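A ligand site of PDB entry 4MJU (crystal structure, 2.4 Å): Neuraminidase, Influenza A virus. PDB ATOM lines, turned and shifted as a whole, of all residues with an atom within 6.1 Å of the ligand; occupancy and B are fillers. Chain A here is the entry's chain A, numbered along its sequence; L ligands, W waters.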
ATOM      1  N   ARG A  36       3.997 -24.730 -17.847  1.00  0.00           N
ATOM      2  CA  ARG A  36       5.260 -25.198 -17.337  1.00  0.00           C
ATOM      3  C   ARG A  36       5.502 -24.364 -16.084  1.00  0.00           C
ATOM      4  O   ARG A  36       4.785 -23.407 -15.827  1.00  0.00           O
ATOM      5  CB  ARG A  36       6.368 -24.936 -18.359  1.00  0.00           C
ATOM      6  CG  ARG A  36       6.453 -25.988 -19.454  1.00  0.00           C
ATOM      7  CD  ARG A  36       7.113 -27.265 -18.943  1.00  0.00           C
ATOM      8  NE  ARG A  36       8.221 -26.981 -18.049  1.00  0.00           N
ATOM      9  CZ  ARG A  36       9.501 -27.140 -18.358  1.00  0.00           C
ATOM     10  NH1 ARG A  36       9.837 -27.586 -19.569  1.00  0.00           N
ATOM     11  NH2 ARG A  36      10.450 -26.861 -17.476  1.00  0.00           N
ATOM     12  N   GLU A  37       6.515 -24.749 -15.300  1.00  0.00           N
ATOM     13  CA  GLU A  37       6.902 -24.027 -14.071  1.00  0.00           C
ATOM     14  C   GLU A  37       5.805 -23.745 -13.046  1.00  0.00           C
ATOM     15  O   GLU A  37       5.568 -22.570 -12.718  1.00  0.00           O
ATOM     16  CB  GLU A  37       7.478 -22.668 -14.412  1.00  0.00           C
ATOM     17  CG  GLU A  37       8.334 -22.618 -15.617  1.00  0.00           C
ATOM     18  CD  GLU A  37       8.938 -21.248 -15.781  1.00  0.00           C
ATOM     19  OE1 GLU A  37       8.465 -20.295 -15.100  1.00  0.00           O
ATOM     20  OE2 GLU A  37       9.879 -21.132 -16.581  1.00  0.00           O
ATOM     21  N   LEU A  52       3.396 -20.565 -16.088  1.00  0.00           N
ATOM     22  CA  LEU A  52       3.446 -19.952 -17.393  1.00  0.00           C
ATOM     23  C   LEU A  52       2.453 -20.624 -18.312  1.00  0.00           C
ATOM     24  O   LEU A  52       2.491 -21.845 -18.489  1.00  0.00           O
ATOM     25  CB  LEU A  52       4.856 -20.046 -17.960  1.00  0.00           C
ATOM     26  CG  LEU A  52       5.855 -19.183 -17.187  1.00  0.00           C
ATOM     27  CD1 LEU A  52       7.219 -19.236 -17.841  1.00  0.00           C
ATOM     28  CD2 LEU A  52       5.335 -17.758 -17.124  1.00  0.00           C
ATOM     29  N   ASP A  69       9.144 -21.279 -27.269  1.00  0.00           N
ATOM     30  CA  ASP A  69       9.066 -21.187 -25.812  1.00  0.00           C
ATOM     31  C   ASP A  69       8.816 -19.747 -25.393  1.00  0.00           C
ATOM     32  O   ASP A  69       7.902 -19.449 -24.620  1.00  0.00           O
ATOM     33  CB  ASP A  69      10.343 -21.709 -25.150  1.00  0.00           C
ATOM     34  CG  ASP A  69      10.452 -23.226 -25.175  1.00  0.00           C
ATOM     35  OD1 ASP A  69       9.405 -23.910 -25.168  1.00  0.00           O
ATOM     36  OD2 ASP A  69      11.586 -23.752 -25.211  1.00  0.00           O
ATOM     37  N   ARG A  70       9.631 -18.838 -25.930  1.00  0.00           N
ATOM     38  CA  ARG A  70       9.490 -17.429 -25.629  1.00  0.00           C
ATOM     39  C   ARG A  70       8.592 -16.744 -26.656  1.00  0.00           C
ATOM     40  O   ARG A  70       9.066 -15.982 -27.503  1.00  0.00           O
ATOM     41  CB  ARG A  70      10.867 -16.788 -25.561  1.00  0.00           C
ATOM     42  CG  ARG A  70      11.779 -17.463 -24.543  1.00  0.00           C
ATOM     43  CD  ARG A  70      13.146 -16.791 -24.459  1.00  0.00           C
ATOM     44  NE  ARG A  70      13.881 -16.936 -25.715  1.00  0.00           N
ATOM     45  CZ  ARG A  70      14.558 -18.027 -26.067  1.00  0.00           C
ATOM     46  NH1 ARG A  70      15.190 -18.055 -27.232  1.00  0.00           N
ATOM     47  NH2 ARG A  70      14.604 -19.078 -25.262  1.00  0.00           N
ATOM     48  N   ARG A  74       2.842 -16.135 -24.061  1.00  0.00           N
ATOM     49  CA  ARG A  74       3.132 -16.623 -22.720  1.00  0.00           C
ATOM     50  C   ARG A  74       2.750 -15.600 -21.663  1.00  0.00           C
ATOM     51  O   ARG A  74       3.048 -14.413 -21.810  1.00  0.00           O
ATOM     52  CB  ARG A  74       4.619 -16.981 -22.592  1.00  0.00           C
ATOM     53  CG  ARG A  74       4.967 -18.363 -23.118  1.00  0.00           C
ATOM     54  CD  ARG A  74       4.604 -19.454 -22.113  1.00  0.00           C
ATOM     55  NE  ARG A  74       5.736 -20.338 -21.839  1.00  0.00           N
ATOM     56  CZ  ARG A  74       5.608 -21.593 -21.424  1.00  0.00           C
ATOM     57  NH1 ARG A  74       6.693 -22.330 -21.192  1.00  0.00           N
ATOM     58  NH2 ARG A  74       4.402 -22.117 -21.238  1.00  0.00           N
ATOM     59  N   TRP A  97       7.535 -14.944 -20.449  1.00  0.00           N
ATOM     60  CA  TRP A  97       8.022 -16.268 -20.787  1.00  0.00           C
ATOM     61  C   TRP A  97       9.120 -16.734 -19.815  1.00  0.00           C
ATOM     62  O   TRP A  97       9.692 -17.814 -19.958  1.00  0.00           O
ATOM     63  CB  TRP A  97       8.444 -16.395 -22.265  1.00  0.00           C
ATOM     64  CG  TRP A  97       9.190 -15.234 -22.871  1.00  0.00           C
ATOM     65  CD1 TRP A  97       8.755 -14.407 -23.868  1.00  0.00           C
ATOM     66  CD2 TRP A  97      10.531 -14.795 -22.568  1.00  0.00           C
ATOM     67  NE1 TRP A  97       9.716 -13.479 -24.188  1.00  0.00           N
ATOM     68  CE2 TRP A  97      10.821 -13.698 -23.404  1.00  0.00           C
ATOM     69  CE3 TRP A  97      11.501 -15.224 -21.645  1.00  0.00           C
ATOM     70  CZ2 TRP A  97      12.037 -13.015 -23.346  1.00  0.00           C
ATOM     71  CZ3 TRP A  97      12.708 -14.546 -21.606  1.00  0.00           C
ATOM     72  CH2 TRP A  97      12.969 -13.452 -22.448  1.00  0.00           C
ATOM     73  N   SER A  98       9.400 -15.890 -18.827  1.00  0.00           N
ATOM     74  CA  SER A  98      10.242 -16.247 -17.687  1.00  0.00           C
ATOM     75  C   SER A  98       9.739 -15.401 -16.517  1.00  0.00           C
ATOM     76  O   SER A  98       9.287 -14.264 -16.736  1.00  0.00           O
ATOM     77  CB  SER A  98      11.727 -15.953 -17.964  1.00  0.00           C
ATOM     78  OG  SER A  98      12.540 -16.297 -16.855  1.00  0.00           O
ATOM     79  N   ALA A  99       9.805 -15.904 -15.297  1.00  0.00           N
ATOM     80  CA  ALA A  99       9.142 -15.198 -14.201  1.00  0.00           C
ATOM     81  C   ALA A  99       9.645 -15.510 -12.795  1.00  0.00           C
ATOM     82  O   ALA A  99      10.228 -16.558 -12.535  1.00  0.00           O
ATOM     83  CB  ALA A  99       7.616 -15.427 -14.270  1.00  0.00           C
ATOM     84  N   ILE A 141      18.599 -13.019 -24.113  1.00  0.00           N
ATOM     85  CA  ILE A 141      17.571 -13.661 -23.306  1.00  0.00           C
ATOM     86  C   ILE A 141      17.656 -13.361 -21.802  1.00  0.00           C
ATOM     87  O   ILE A 141      17.980 -14.239 -21.004  1.00  0.00           O
ATOM     88  CB  ILE A 141      17.592 -15.186 -23.553  1.00  0.00           C
ATOM     89  CG1 ILE A 141      17.721 -15.480 -25.040  1.00  0.00           C
ATOM     90  CG2 ILE A 141      16.322 -15.842 -23.018  1.00  0.00           C
ATOM     91  CD1 ILE A 141      17.712 -16.964 -25.352  1.00  0.00           C
ATOM     92  N   LEU A 142      17.370 -12.123 -21.439  1.00  0.00           N
ATOM     93  CA  LEU A 142      17.147 -11.761 -20.041  1.00  0.00           C
ATOM     94  C   LEU A 142      16.132 -12.737 -19.437  1.00  0.00           C
ATOM     95  O   LEU A 142      15.156 -13.104 -20.097  1.00  0.00           O
ATOM     96  CB  LEU A 142      16.609 -10.332 -19.940  1.00  0.00           C
ATOM     97  CG  LEU A 142      16.271  -9.827 -18.546  1.00  0.00           C
ATOM     98  CD1 LEU A 142      17.534  -9.744 -17.710  1.00  0.00           C
ATOM     99  CD2 LEU A 142      15.611  -8.477 -18.646  1.00  0.00           C
ATOM    100  N   ARG A 143      16.421 -13.213 -18.231  1.00  0.00           N
ATOM    101  CA  ARG A 143      15.628 -14.271 -17.609  1.00  0.00           C
ATOM    102  C   ARG A 143      15.870 -14.379 -16.108  1.00  0.00           C
ATOM    103  O   ARG A 143      16.952 -14.055 -15.607  1.00  0.00           O
ATOM    104  CB  ARG A 143      15.904 -15.613 -18.283  1.00  0.00           C
ATOM    105  CG  ARG A 143      17.364 -16.046 -18.232  1.00  0.00           C
ATOM    106  CD  ARG A 143      17.651 -17.136 -19.251  1.00  0.00           C
ATOM    107  NE  ARG A 143      19.033 -17.596 -19.181  1.00  0.00           N
ATOM    108  CZ  ARG A 143      20.038 -17.069 -19.872  1.00  0.00           C
ATOM    109  NH1 ARG A 143      21.265 -17.556 -19.749  1.00  0.00           N
ATOM    110  NH2 ARG A 143      19.810 -16.056 -20.698  1.00  0.00           N
ATOM    111  N   GLU A 146      12.092 -18.692 -12.259  1.00  0.00           N
ATOM    112  CA  GLU A 146      10.991 -19.664 -12.341  1.00  0.00           C
ATOM    113  C   GLU A 146      10.625 -20.336 -11.010  1.00  0.00           C
ATOM    114  O   GLU A 146      10.200 -21.482 -10.990  1.00  0.00           O
ATOM    115  CB  GLU A 146      11.306 -20.701 -13.429  1.00  0.00           C
ATOM    116  CG  GLU A 146      12.183 -20.198 -14.589  1.00  0.00           C
ATOM    117  CD  GLU A 146      11.532 -19.104 -15.444  1.00  0.00           C
ATOM    118  OE1 GLU A 146      10.526 -18.505 -15.014  1.00  0.00           O
ATOM    119  OE2 GLU A 146      12.026 -18.858 -16.570  1.00  0.00           O
ATOM    120  N   ALA A 165      23.339 -19.581 -22.667  1.00  0.00           N
ATOM    121  CA  ALA A 165      22.830 -20.617 -21.784  1.00  0.00           C
ATOM    122  C   ALA A 165      23.724 -21.866 -21.705  1.00  0.00           C
ATOM    123  O   ALA A 165      23.437 -22.792 -20.937  1.00  0.00           O
ATOM    124  CB  ALA A 165      21.440 -21.017 -22.223  1.00  0.00           C
ATOM    125  N   HIS A 193      28.311 -20.897 -13.817  1.00  0.00           N
ATOM    126  CA  HIS A 193      27.091 -20.638 -14.564  1.00  0.00           C
ATOM    127  C   HIS A 193      25.872 -20.616 -13.641  1.00  0.00           C
ATOM    128  O   HIS A 193      25.687 -21.538 -12.840  1.00  0.00           O
ATOM    129  CB  HIS A 193      26.912 -21.703 -15.651  1.00  0.00           C
ATOM    130  CG  HIS A 193      26.006 -21.287 -16.764  1.00  0.00           C
ATOM    131  ND1 HIS A 193      24.722 -21.776 -16.909  1.00  0.00           N
ATOM    132  CD2 HIS A 193      26.194 -20.408 -17.773  1.00  0.00           C
ATOM    133  CE1 HIS A 193      24.172 -21.232 -17.978  1.00  0.00           C
ATOM    134  NE2 HIS A 193      25.038 -20.392 -18.509  1.00  0.00           N
ATOM    135  N   GLU A 195      21.669 -20.300 -13.489  1.00  0.00           N
ATOM    136  CA  GLU A 195      20.340 -20.275 -14.082  1.00  0.00           C
ATOM    137  C   GLU A 195      19.300 -20.664 -13.048  1.00  0.00           C
ATOM    138  O   GLU A 195      19.577 -21.494 -12.166  1.00  0.00           O
ATOM    139  CB  GLU A 195      20.219 -21.283 -15.232  1.00  0.00           C
ATOM    140  CG  GLU A 195      21.243 -21.098 -16.336  1.00  0.00           C
ATOM    141  CD  GLU A 195      20.843 -20.014 -17.344  1.00  0.00           C
ATOM    142  OE1 GLU A 195      21.434 -19.995 -18.438  1.00  0.00           O
ATOM    143  OE2 GLU A 195      19.940 -19.202 -17.039  1.00  0.00           O
ATOM    144  N   GLU A 196      18.112 -20.060 -13.179  1.00  0.00           N
ATOM    145  CA  GLU A 196      16.901 -20.542 -12.518  1.00  0.00           C
ATOM    146  C   GLU A 196      17.063 -20.829 -11.035  1.00  0.00           C
ATOM    147  O   GLU A 196      16.854 -21.966 -10.597  1.00  0.00           O
ATOM    148  CB  GLU A 196      16.433 -21.812 -13.233  1.00  0.00           C
ATOM    149  CG  GLU A 196      15.968 -21.538 -14.665  1.00  0.00           C
ATOM    150  CD  GLU A 196      15.721 -22.796 -15.494  1.00  0.00           C
ATOM    151  OE1 GLU A 196      16.265 -23.872 -15.157  1.00  0.00           O
ATOM    152  OE2 GLU A 196      14.988 -22.697 -16.491  1.00  0.00           O
ATOM    153  N   ARG A 211      21.127 -23.599 -11.060  1.00  0.00           N
ATOM    154  CA  ARG A 211      21.386 -24.555 -12.127  1.00  0.00           C
ATOM    155  C   ARG A 211      22.555 -24.059 -12.981  1.00  0.00           C
ATOM    156  O   ARG A 211      22.511 -22.952 -13.537  1.00  0.00           O
ATOM    157  CB  ARG A 211      20.127 -24.737 -12.976  1.00  0.00           C
ATOM    158  CG  ARG A 211      20.333 -25.404 -14.342  1.00  0.00           C
ATOM    159  CD  ARG A 211      19.029 -25.401 -15.149  1.00  0.00           C
ATOM    160  NE  ARG A 211      19.187 -25.879 -16.514  1.00  0.00           N
ATOM    161  CZ  ARG A 211      18.168 -26.087 -17.364  1.00  0.00           C
ATOM    162  NH1 ARG A 211      18.409 -26.538 -18.596  1.00  0.00           N
ATOM    163  NH2 ARG A 211      16.915 -25.840 -16.986  1.00  0.00           N
ATOM    164  N   ASN A 213      24.259 -24.661 -16.322  1.00  0.00           N
ATOM    165  CA  ASN A 213      23.881 -25.240 -17.598  1.00  0.00           C
ATOM    166  C   ASN A 213      25.076 -25.354 -18.549  1.00  0.00           C
ATOM    167  O   ASN A 213      24.920 -25.676 -19.723  1.00  0.00           O
ATOM    168  CB  ASN A 213      22.771 -24.378 -18.238  1.00  0.00           C
ATOM    169  CG  ASN A 213      21.806 -25.205 -19.068  1.00  0.00           C
ATOM    170  OD1 ASN A 213      21.283 -26.210 -18.611  1.00  0.00           O
ATOM    171  ND2 ASN A 213      21.581 -24.782 -20.318  1.00  0.00           N
ATOM    172  N   TYR A 264      24.046 -29.022 -20.131  1.00  0.00           N
ATOM    173  CA  TYR A 264      22.642 -29.111 -19.768  1.00  0.00           C
ATOM    174  C   TYR A 264      22.427 -28.994 -18.260  1.00  0.00           C
ATOM    175  O   TYR A 264      23.349 -28.677 -17.505  1.00  0.00           O
ATOM    176  CB  TYR A 264      22.044 -30.414 -20.275  1.00  0.00           C
ATOM    177  CG  TYR A 264      20.562 -30.320 -20.608  1.00  0.00           C
ATOM    178  CD1 TYR A 264      20.090 -29.315 -21.432  1.00  0.00           C
ATOM    179  CD2 TYR A 264      19.657 -31.240 -20.113  1.00  0.00           C
ATOM    180  CE1 TYR A 264      18.745 -29.221 -21.747  1.00  0.00           C
ATOM    181  CE2 TYR A 264      18.318 -31.163 -20.415  1.00  0.00           C
ATOM    182  CZ  TYR A 264      17.863 -30.147 -21.225  1.00  0.00           C
ATOM    183  OH  TYR A 264      16.525 -30.059 -21.536  1.00  0.00           O
ATOM    184  N   GLY A 265      21.197 -29.258 -17.839  1.00  0.00           N
ATOM    185  CA  GLY A 265      20.802 -29.154 -16.449  1.00  0.00           C
ATOM    186  C   GLY A 265      19.294 -29.196 -16.296  1.00  0.00           C
ATOM    187  O   GLY A 265      18.558 -29.403 -17.262  1.00  0.00           O
ATOM    188  N   VAL A 266      18.829 -29.023 -15.062  1.00  0.00           N
ATOM    189  CA  VAL A 266      17.415 -28.911 -14.775  1.00  0.00           C
ATOM    190  C   VAL A 266      17.348 -28.006 -13.557  1.00  0.00           C
ATOM    191  O   VAL A 266      18.253 -28.032 -12.728  1.00  0.00           O
ATOM    192  CB  VAL A 266      16.767 -30.290 -14.521  1.00  0.00           C
ATOM    193  CG1 VAL A 266      17.371 -31.001 -13.295  1.00  0.00           C
ATOM    194  CG2 VAL A 266      15.228 -30.163 -14.405  1.00  0.00           C
ATOM    195  N   ARG A 288      14.691 -36.728 -16.812  1.00  0.00           N
ATOM    196  CA  ARG A 288      13.853 -36.052 -15.844  1.00  0.00           C
ATOM    197  C   ARG A 288      12.709 -36.961 -15.425  1.00  0.00           C
ATOM    198  O   ARG A 288      11.541 -36.743 -15.782  1.00  0.00           O
ATOM    199  CB  ARG A 288      13.316 -34.755 -16.439  1.00  0.00           C
ATOM    200  CG  ARG A 288      14.414 -33.761 -16.714  1.00  0.00           C
ATOM    201  CD  ARG A 288      13.935 -32.636 -17.591  1.00  0.00           C
ATOM    202  NE  ARG A 288      14.911 -31.558 -17.585  1.00  0.00           N
ATOM    203  CZ  ARG A 288      14.679 -30.332 -18.028  1.00  0.00           C
ATOM    204  NH1 ARG A 288      15.652 -29.436 -17.946  1.00  0.00           N
ATOM    205  NH2 ARG A 288      13.489 -30.002 -18.531  1.00  0.00           N
ATOM    206  N   TYR A 322      11.259 -29.730 -13.426  1.00  0.00           N
ATOM    207  CA  TYR A 322      11.707 -28.666 -12.540  1.00  0.00           C
ATOM    208  C   TYR A 322      11.337 -28.910 -11.079  1.00  0.00           C
ATOM    209  O   TYR A 322      10.353 -29.609 -10.765  1.00  0.00           O
ATOM    210  CB  TYR A 322      11.151 -27.310 -13.000  1.00  0.00           C
ATOM    211  CG  TYR A 322      11.941 -26.624 -14.098  1.00  0.00           C
ATOM    212  CD1 TYR A 322      12.880 -27.322 -14.835  1.00  0.00           C
ATOM    213  CD2 TYR A 322      11.746 -25.273 -14.377  1.00  0.00           C
ATOM    214  CE1 TYR A 322      13.615 -26.714 -15.828  1.00  0.00           C
ATOM    215  CE2 TYR A 322      12.474 -24.653 -15.365  1.00  0.00           C
ATOM    216  CZ  TYR A 322      13.412 -25.380 -16.093  1.00  0.00           C
ATOM    217  OH  TYR A 322      14.153 -24.778 -17.082  1.00  0.00           O
ATOM    218  N   ILE A 347       6.410 -33.233 -15.855  1.00  0.00           N
ATOM    219  CA  ILE A 347       6.205 -32.934 -17.267  1.00  0.00           C
ATOM    220  C   ILE A 347       5.632 -34.111 -18.062  1.00  0.00           C
ATOM    221  O   ILE A 347       6.171 -35.222 -18.038  1.00  0.00           O
ATOM    222  CB  ILE A 347       7.525 -32.431 -17.907  1.00  0.00           C
ATOM    223  CG1 ILE A 347       8.084 -31.253 -17.110  1.00  0.00           C
ATOM    224  CG2 ILE A 347       7.319 -32.082 -19.394  1.00  0.00           C
ATOM    225  CD1 ILE A 347       9.409 -30.705 -17.634  1.00  0.00           C
HETATM  226  O1  LIG L   1      11.265 -23.187 -22.084  1.00  0.00           O
HETATM  227  C1  LIG L   1      11.503 -22.666 -20.996  1.00  0.00           C
HETATM  228  N1  LIG L   1      10.673 -21.737 -20.500  1.00  0.00           N
HETATM  229  C2  LIG L   1      11.043 -21.264 -19.306  1.00  0.00           C
HETATM  230  N2  LIG L   1      10.717 -20.071 -18.841  1.00  0.00           N
HETATM  231  S1  LIG L   1      12.024 -22.385 -18.566  1.00  0.00           S
HETATM  232  C3  LIG L   1      12.630 -22.990 -20.186  1.00  0.00           C
HETATM  233  C4  LIG L   1      13.894 -22.280 -20.673  1.00  0.00           C
HETATM  234  N3  LIG L   1      13.798 -20.856 -20.351  1.00  0.00           N
HETATM  235  C5  LIG L   1      13.640 -19.917 -21.295  1.00  0.00           C
HETATM  236  O2  LIG L   1      13.559 -20.171 -22.494  1.00  0.00           O
HETATM  237  C6  LIG L   1      13.553 -18.475 -20.774  1.00  0.00           C
HETATM  238  C7  LIG L   1      12.811 -24.378 -20.155  1.00  0.00           C
HETATM  239  C8  LIG L   1      14.050 -25.033 -20.146  1.00  0.00           C
HETATM  240  C9  LIG L   1      14.090 -26.378 -19.762  1.00  0.00           C
HETATM  241  O3  LIG L   1      13.027 -27.025 -19.615  1.00  0.00           O
HETATM  242  O4  LIG L   1      15.178 -26.960 -19.571  1.00  0.00           O
HETATM  243  C10 LIG L   1      15.260 -24.319 -20.211  1.00  0.00           C
HETATM  244  C11 LIG L   1      15.128 -22.821 -19.991  1.00  0.00           C
HETATM  245  O5  LIG L   1      16.278 -22.144 -20.539  1.00  0.00           O
HETATM  246  C12 LIG L   1      16.993 -21.360 -19.565  1.00  0.00           C
HETATM  247  C13 LIG L   1      17.560 -22.251 -18.437  1.00  0.00           C
HETATM  248  C14 LIG L   1      18.899 -22.894 -18.829  1.00  0.00           C
HETATM  249  C15 LIG L   1      18.141 -20.589 -20.246  1.00  0.00           C
HETATM  250  C16 LIG L   1      17.603 -19.802 -21.439  1.00  0.00           C
HETATM  251  O   HOH W   1      14.245 -20.255 -17.472  1.00  0.00           O
HETATM  252  O   HOH W   2       8.987 -23.865 -19.333  1.00  0.00           O
HETATM  253  O   HOH W   3      17.898 -23.113 -22.932  1.00  0.00           O
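The side-chain carboxylate of Glu 146 is in hydrogen-bond range of the side-chain hydroxyl of Ser 98 (2.6 Å).
The backbone carbonyl oxygen of Arg 36 is in hydrogen-bond range of the backbone NH of Leu 52 (3.2 Å).
OE1 of Glu 196 lies within salt-bridge range of NH2 of Arg 211, 2.8 Å away.
The backbone carbonyl oxygen (O) of Ile 141 is in hydrogen-bond range of the guanidinium group (NH2) of Arg 143 (2.6 Å).
O of Arg 211 sits at hydrogen-bond distance from N of Glu 195 (2.8 Å).
NH1 of Arg 211 is in hydrogen-bond range of O of Gly 265 (3.2 Å).
The backbone NH (N) of Asn 213 lies within hydrogen-bond range of a ring nitrogen (ND1) of His 193, 3.0 Å away.
O of Leu 52 is in hydrogen-bond range of NH2 of Arg 74, 3.4 Å away.
Water W2 lies within hydrogen-bond range of a nitrogen (N1) of the ligand (3.0 Å), the guanidinium group of Arg 74 (3.3 Å) and the guanidinium group of Arg 36 (3.5 Å).
Water W1 lies within hydrogen-bond range of OE2 of Glu 196 (2.7 Å), OE2 of Glu 146 (2.8 Å) and N3 of the ligand (3.0 Å).
The side-chain carboxylate (OE2) of Glu 37 is in hydrogen-bond range of a nitrogen (N2) of the ligand, 2.6 Å away.
A nitrogen (N2) of the ligand sits at hydrogen-bond distance from the backbone carbonyl oxygen (O) of Trp 97, 2.7 Å away.
A nitrogen (N2) of the ligand is in hydrogen-bond range of the side-chain carboxylate (OE2) of Glu 146, 2.9 Å away.
The guanidinium group of Arg 288 lies within salt-bridge range of an oxygen (O4) of the ligand (3.0 Å).
The side-chain hydroxyl (OH) of Tyr 322 lies close to an oxygen (O4) of the ligand.
O2 of the ligand is in hydrogen-bond range of NH2 of Arg 70 (3.2 Å).
The guanidinium group of Arg 36 lies within salt-bridge range of an oxygen (O3) of the ligand (3.2 Å).
An oxygen (O4) of the ligand lies within salt-bridge range of the guanidinium group (NH2) of Arg 211, at 3.3 Å.
OD2 of Asp 69 sits close to O1 of the ligand (3.2 Å).
OE2 of Glu 196 lies close to S1 of the ligand.
Leu 52 touches the ligand.
NE of Arg 143 touches C15 of the ligand, 3.3 Å away.
CB of Ala 165 touches C15 of the ligand, 3.9 Å away.
CD of Glu 195 touches C14 of the ligand, at 3.8 Å.
Asn 213 touches the ligand (ND2 to C14, 3.6 Å).
Tyr 264 touches the ligand (OH to O4, 3.9 Å).
Hydrophobic or aromatic side chains that line the ligand: Leu 52, Trp 97, Ala 165 and Tyr 322.
Of the 25 residues printed, 16 come within 4 Å of the ligand.
Along chain A the residues within 4 Å of the ligand span positions 36 to 322.
The nearest printed residue that does not touch the ligand is Ser 98 (4.02 Å).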
